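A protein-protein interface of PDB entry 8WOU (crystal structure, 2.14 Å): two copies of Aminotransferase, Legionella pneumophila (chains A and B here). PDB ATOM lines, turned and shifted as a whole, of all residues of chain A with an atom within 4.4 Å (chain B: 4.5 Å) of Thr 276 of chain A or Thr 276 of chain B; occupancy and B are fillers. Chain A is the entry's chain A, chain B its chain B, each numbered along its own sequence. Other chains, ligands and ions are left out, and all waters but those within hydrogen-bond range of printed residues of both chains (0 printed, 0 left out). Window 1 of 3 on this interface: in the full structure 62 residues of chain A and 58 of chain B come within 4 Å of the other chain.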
ATOM      1  N   VAL A 106      20.305  -8.320   8.135  1.00  0.00           N
ATOM      2  CA  VAL A 106      20.191  -9.776   7.997  1.00  0.00           C
ATOM      3  C   VAL A 106      21.302 -10.388   8.837  1.00  0.00           C
ATOM      4  O   VAL A 106      22.386 -10.742   8.335  1.00  0.00           O
ATOM      5  CB  VAL A 106      20.265 -10.221   6.542  1.00  0.00           C
ATOM      6  CG1 VAL A 106      20.013 -11.708   6.457  1.00  0.00           C
ATOM      7  CG2 VAL A 106      19.249  -9.470   5.707  1.00  0.00           C
ATOM      8  N   GLN A 110      25.891  -8.968   9.182  1.00  0.00           N
ATOM      9  CA  GLN A 110      25.699  -8.045   8.071  1.00  0.00           C
ATOM     10  C   GLN A 110      25.754  -6.593   8.523  1.00  0.00           C
ATOM     11  O   GLN A 110      26.338  -5.755   7.828  1.00  0.00           O
ATOM     12  CB  GLN A 110      24.382  -8.327   7.352  1.00  0.00           C
ATOM     13  CG  GLN A 110      24.328  -7.526   6.067  1.00  0.00           C
ATOM     14  CD  GLN A 110      22.968  -7.447   5.459  1.00  0.00           C
ATOM     15  OE1 GLN A 110      21.960  -7.528   6.154  1.00  0.00           O
ATOM     16  NE2 GLN A 110      22.924  -7.258   4.145  1.00  0.00           N
ATOM     17  N   ARG A 254      18.422 -14.891  11.374  1.00  0.00           N
ATOM     18  CA  ARG A 254      19.192 -13.880  10.642  1.00  0.00           C
ATOM     19  C   ARG A 254      18.563 -12.485  10.760  1.00  0.00           C
ATOM     20  O   ARG A 254      18.253 -11.831   9.760  1.00  0.00           O
ATOM     21  CB  ARG A 254      19.382 -14.258   9.157  1.00  0.00           C
ATOM     22  CG  ARG A 254      19.645 -15.741   8.817  1.00  0.00           C
ATOM     23  CD  ARG A 254      20.990 -16.292   9.337  1.00  0.00           C
ATOM     24  NE  ARG A 254      22.098 -15.338   9.239  1.00  0.00           N
ATOM     25  CZ  ARG A 254      22.755 -14.849  10.295  1.00  0.00           C
ATOM     26  NH1 ARG A 254      22.411 -15.229  11.523  1.00  0.00           N
ATOM     27  NH2 ARG A 254      23.749 -13.972  10.134  1.00  0.00           N
ATOM     28  N   GLN A 272      22.827  -1.968   1.988  1.00  0.00           N
ATOM     29  CA  GLN A 272      21.913  -3.081   2.215  1.00  0.00           C
ATOM     30  C   GLN A 272      20.858  -3.171   1.124  1.00  0.00           C
ATOM     31  O   GLN A 272      20.511  -4.271   0.691  1.00  0.00           O
ATOM     32  CB  GLN A 272      21.242  -2.939   3.581  1.00  0.00           C
ATOM     33  CG  GLN A 272      20.293  -4.070   3.914  1.00  0.00           C
ATOM     34  CD  GLN A 272      19.973  -4.115   5.395  1.00  0.00           C
ATOM     35  OE1 GLN A 272      20.873  -4.030   6.237  1.00  0.00           O
ATOM     36  NE2 GLN A 272      18.690  -4.234   5.723  1.00  0.00           N
ATOM     37  N   GLN A 274      21.234  -2.525  -1.880  1.00  0.00           N
ATOM     38  CA  GLN A 274      21.892  -3.017  -3.077  1.00  0.00           C
ATOM     39  C   GLN A 274      22.545  -4.378  -2.864  1.00  0.00           C
ATOM     40  O   GLN A 274      23.367  -4.790  -3.676  1.00  0.00           O
ATOM     41  CB  GLN A 274      22.922  -1.994  -3.552  1.00  0.00           C
ATOM     42  CG  GLN A 274      22.306  -0.627  -3.904  1.00  0.00           C
ATOM     43  CD  GLN A 274      21.190  -0.704  -4.967  1.00  0.00           C
ATOM     44  OE1 GLN A 274      21.096  -1.666  -5.733  1.00  0.00           O
ATOM     45  NE2 GLN A 274      20.346   0.322  -5.011  1.00  0.00           N
ATOM     46  N   SER A 275      22.213  -5.081  -1.786  1.00  0.00           N
ATOM     47  CA  SER A 275      22.814  -6.397  -1.579  1.00  0.00           C
ATOM     48  C   SER A 275      21.755  -7.402  -1.165  1.00  0.00           C
ATOM     49  O   SER A 275      21.557  -8.407  -1.846  1.00  0.00           O
ATOM     50  CB  SER A 275      23.944  -6.350  -0.546  1.00  0.00           C
ATOM     51  OG  SER A 275      23.567  -5.615   0.609  1.00  0.00           O
ATOM     52  N   THR A 276      21.045  -7.152  -0.076  1.00  0.00           N
ATOM     53  CA  THR A 276      20.005  -8.081   0.340  1.00  0.00           C
ATOM     54  C   THR A 276      18.602  -7.506   0.245  1.00  0.00           C
ATOM     55  O   THR A 276      17.637  -8.277   0.286  1.00  0.00           O
ATOM     56  CB  THR A 276      20.247  -8.536   1.785  1.00  0.00           C
ATOM     57  OG1 THR A 276      20.310  -7.376   2.619  1.00  0.00           O
ATOM     58  CG2 THR A 276      21.573  -9.305   1.894  1.00  0.00           C
ATOM     59  N   SER A 277      18.470  -6.198   0.083  1.00  0.00           N
ATOM     60  CA  SER A 277      17.278  -5.438   0.467  1.00  0.00           C
ATOM     61  C   SER A 277      16.855  -5.902   1.873  1.00  0.00           C
ATOM     62  O   SER A 277      17.697  -6.219   2.720  1.00  0.00           O
ATOM     63  CB  SER A 277      16.207  -5.550  -0.601  1.00  0.00           C
ATOM     64  OG  SER A 277      15.513  -6.774  -0.493  1.00  0.00           O
ATOM     65  N   ASN A 278      15.554  -5.941   2.146  1.00  0.00           N
ATOM     66  CA  ASN A 278      15.075  -6.116   3.509  1.00  0.00           C
ATOM     67  C   ASN A 278      15.319  -7.542   3.986  1.00  0.00           C
ATOM     68  O   ASN A 278      15.463  -8.464   3.184  1.00  0.00           O
ATOM     69  CB  ASN A 278      13.590  -5.781   3.584  1.00  0.00           C
ATOM     70  CG  ASN A 278      12.730  -6.740   2.773  1.00  0.00           C
ATOM     71  OD1 ASN A 278      12.480  -6.512   1.598  1.00  0.00           O
ATOM     72  ND2 ASN A 278      12.289  -7.827   3.400  1.00  0.00           N
ATOM     73  N   VAL B 106      20.751 -14.742  -0.096  1.00  0.00           N
ATOM     74  CA  VAL B 106      19.668 -14.026   0.581  1.00  0.00           C
ATOM     75  C   VAL B 106      18.929 -13.169  -0.428  1.00  0.00           C
ATOM     76  O   VAL B 106      19.127 -11.947  -0.497  1.00  0.00           O
ATOM     77  CB  VAL B 106      20.197 -13.167   1.746  1.00  0.00           C
ATOM     78  CG1 VAL B 106      19.040 -12.603   2.550  1.00  0.00           C
ATOM     79  CG2 VAL B 106      21.116 -13.987   2.642  1.00  0.00           C
ATOM     80  N   GLN B 110      21.165 -10.634  -3.781  1.00  0.00           N
ATOM     81  CA  GLN B 110      22.449 -10.932  -3.140  1.00  0.00           C
ATOM     82  C   GLN B 110      23.338 -11.821  -4.001  1.00  0.00           C
ATOM     83  O   GLN B 110      24.569 -11.696  -3.945  1.00  0.00           O
ATOM     84  CB  GLN B 110      22.259 -11.585  -1.779  1.00  0.00           C
ATOM     85  CG  GLN B 110      23.560 -11.486  -0.947  1.00  0.00           C
ATOM     86  CD  GLN B 110      23.665 -12.517   0.151  1.00  0.00           C
ATOM     87  OE1 GLN B 110      23.014 -13.550   0.109  1.00  0.00           O
ATOM     88  NE2 GLN B 110      24.484 -12.233   1.154  1.00  0.00           N
ATOM     89  N   ARG B 254      13.218 -13.824   0.694  1.00  0.00           N
ATOM     90  CA  ARG B 254      14.652 -13.574   0.486  1.00  0.00           C
ATOM     91  C   ARG B 254      15.441 -14.863   0.204  1.00  0.00           C
ATOM     92  O   ARG B 254      16.398 -15.197   0.903  1.00  0.00           O
ATOM     93  CB  ARG B 254      15.285 -12.823   1.677  1.00  0.00           C
ATOM     94  CG  ARG B 254      14.467 -11.706   2.318  1.00  0.00           C
ATOM     95  CD  ARG B 254      13.957 -10.650   1.308  1.00  0.00           C
ATOM     96  NE  ARG B 254      15.033 -10.084   0.497  1.00  0.00           N
ATOM     97  CZ  ARG B 254      15.203 -10.311  -0.806  1.00  0.00           C
ATOM     98  NH1 ARG B 254      14.364 -11.082  -1.480  1.00  0.00           N
ATOM     99  NH2 ARG B 254      16.211  -9.746  -1.440  1.00  0.00           N
ATOM    100  N   GLN B 272      29.872 -14.301   1.005  1.00  0.00           N
ATOM    101  CA  GLN B 272      28.651 -14.513   1.768  1.00  0.00           C
ATOM    102  C   GLN B 272      28.967 -14.911   3.207  1.00  0.00           C
ATOM    103  O   GLN B 272      28.347 -14.401   4.147  1.00  0.00           O
ATOM    104  CB  GLN B 272      27.795 -15.568   1.069  1.00  0.00           C
ATOM    105  CG  GLN B 272      26.383 -15.761   1.617  1.00  0.00           C
ATOM    106  CD  GLN B 272      25.485 -16.465   0.613  1.00  0.00           C
ATOM    107  OE1 GLN B 272      25.363 -16.033  -0.526  1.00  0.00           O
ATOM    108  NE2 GLN B 272      24.848 -17.535   1.033  1.00  0.00           N
ATOM    109  N   GLN B 274      31.200 -13.911   4.992  1.00  0.00           N
ATOM    110  CA  GLN B 274      31.668 -12.749   5.725  1.00  0.00           C
ATOM    111  C   GLN B 274      30.675 -11.591   5.705  1.00  0.00           C
ATOM    112  O   GLN B 274      31.032 -10.484   6.117  1.00  0.00           O
ATOM    113  CB  GLN B 274      33.026 -12.295   5.188  1.00  0.00           C
ATOM    114  CG  GLN B 274      34.116 -13.353   5.285  1.00  0.00           C
ATOM    115  CD  GLN B 274      34.552 -13.693   6.714  1.00  0.00           C
ATOM    116  OE1 GLN B 274      34.039 -13.155   7.693  1.00  0.00           O
ATOM    117  NE2 GLN B 274      35.514 -14.607   6.826  1.00  0.00           N
ATOM    118  N   SER B 275      29.430 -11.816   5.261  1.00  0.00           N
ATOM    119  CA  SER B 275      28.431 -10.751   5.240  1.00  0.00           C
ATOM    120  C   SER B 275      27.109 -11.181   5.863  1.00  0.00           C
ATOM    121  O   SER B 275      26.709 -10.623   6.885  1.00  0.00           O
ATOM    122  CB  SER B 275      28.193 -10.230   3.813  1.00  0.00           C
ATOM    123  OG  SER B 275      27.889 -11.273   2.897  1.00  0.00           O
ATOM    124  N   THR B 276      26.412 -12.158   5.289  1.00  0.00           N
ATOM    125  CA  THR B 276      25.132 -12.588   5.855  1.00  0.00           C
ATOM    126  C   THR B 276      25.148 -13.944   6.539  1.00  0.00           C
ATOM    127  O   THR B 276      24.170 -14.275   7.217  1.00  0.00           O
ATOM    128  CB  THR B 276      24.080 -12.712   4.763  1.00  0.00           C
ATOM    129  OG1 THR B 276      24.589 -13.687   3.843  1.00  0.00           O
ATOM    130  CG2 THR B 276      23.829 -11.368   4.100  1.00  0.00           C
ATOM    131  N   SER B 277      26.169 -14.760   6.308  1.00  0.00           N
ATOM    132  CA  SER B 277      26.111 -16.205   6.557  1.00  0.00           C
ATOM    133  C   SER B 277      24.942 -16.794   5.763  1.00  0.00           C
ATOM    134  O   SER B 277      24.500 -16.226   4.761  1.00  0.00           O
ATOM    135  CB  SER B 277      26.060 -16.474   8.047  1.00  0.00           C
ATOM    136  OG  SER B 277      27.297 -16.148   8.647  1.00  0.00           O
ATOM    137  N   ASN B 278      24.429 -17.937   6.209  1.00  0.00           N
ATOM    138  CA  ASN B 278      23.368 -18.628   5.494  1.00  0.00           C
ATOM    139  C   ASN B 278      22.087 -17.796   5.493  1.00  0.00           C
ATOM    140  O   ASN B 278      21.824 -17.045   6.431  1.00  0.00           O
ATOM    141  CB  ASN B 278      23.085 -19.979   6.146  1.00  0.00           C
ATOM    142  CG  ASN B 278      22.684 -19.839   7.603  1.00  0.00           C
ATOM    143  OD1 ASN B 278      23.526 -19.595   8.470  1.00  0.00           O
ATOM    144  ND2 ASN B 278      21.387 -19.962   7.876  1.00  0.00           N
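Thr 276 of chain A touches just these residues of chain B: Arg 254 and Thr 276.
Printed residues of chain B within 4 Å of Ser 275 of chain A: Gln 110 (3.0 Å).
Printed residues of chain A within 4 Å of Ser 277 of chain B: Arg 254 (3.99 Å).
Of the printed residues of chain A, Arg 254 of chain B touches Thr 276 (2.7 Å), Ser 277 (3.2 Å) and Asn 278 (3.2 Å).
Printed residues of chain B within 4 Å of Gln 110 of chain A: Ser 275 (2.9 Å).
Printed residues of chain B within 4 Å of Asn 278 of chain A: Arg 254.
The nearest residue of chain A that does not touch Thr 276 of chain B is Val 106 of chain A (4.1 Å).
The nearest printed residue of chain A that does not touch Ser 277 of chain B is Val 106 of chain A (5.9 Å).
Arg 254 of chain A touches Ser 277 of chain B.
CG2 of Thr 276 of chain A touches CG2 of Thr 276 of chain B, 3.8 Å away.
Gln 110 of chain A touches Ser 275 of chain B, and with the chains exchanged Ser 275 of chain A touches Gln 110 of chain B.
Arg 254 of chain A touches Thr 276 of chain B, and with the chains exchanged Thr 276 of chain A touches Arg 254 of chain B.
Arg 254 of chain A touches Ser 277 of chain B, and with the chains exchanged Ser 277 of chain A touches Arg 254 of chain B.
Thr 276 of chain B touches its own counterpart, Thr 276 of chain A.
9 positions are printed for both chains.
The guanidinium group (NH2) of Arg 254 of chain A is in hydrogen-bond range of the backbone carbonyl oxygen (O) of Thr 276 of chain B, at 3.0 Å.
The guanidinium group of Arg 254 of chain A sits close to the backbone carbonyl oxygen of Asn 278 of chain B, 3.3 Å away.
The backbone carbonyl oxygen (O) of Thr 276 of chain A sits at hydrogen-bond distance from the guanidinium group (NH2) of Arg 254 of chain B (2.7 Å).
O of Asn 278 of chain A is in hydrogen-bond range of NE of Arg 254 of chain B (3.2 Å).
N of Gln 110 of chain A sits at hydrogen-bond distance from O of Ser 275 of chain B.
The guanidinium group (NH2) of Arg 254 of chain B lies within hydrogen-bond range of the side-chain hydroxyl (OG) of Ser 277 of chain A (3.2 Å).
The backbone NH of Gln 110 of chain B lies close to the backbone carbonyl oxygen of Ser 275 of chain A, at 3.0 Å.
N of Ser 277 of chain B sits at hydrogen-bond distance from O of Gln 272 of chain B, at 3.1 Å.
O of Gln 272 of chain A sits at hydrogen-bond distance from N of Ser 277 of chain A, at 2.9 Å.
The side-chain amide nitrogen of Gln 110 of chain A sits at hydrogen-bond distance from the side-chain hydroxyl of Thr 276 of chain A, 3.0 Å away.
OE1 of Gln 110 of chain B lies close to OE1 of Gln 272 of chain B, at 3.5 Å.
The backbone NH of Val 106 of chain A sits at hydrogen-bond distance from the side-chain amide oxygen of Gln 110 of chain A (2.7 Å).
O of Gln 272 of chain B is in hydrogen-bond range of OG of Ser 275 of chain B (3.4 Å).
Of the 9 printed residues of chain A, 6 touch a printed residue of chain B.
Printed residues of chain A that touch a printed residue of chain B: Gln 110, Arg 254, Ser 275, Thr 276, Ser 277 and Asn 278.
Along chain A the printed residues that touch a printed residue of chain B span positions 110 to 278.
Of the 9 printed residues of chain B, 6 touch a printed residue of chain A.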
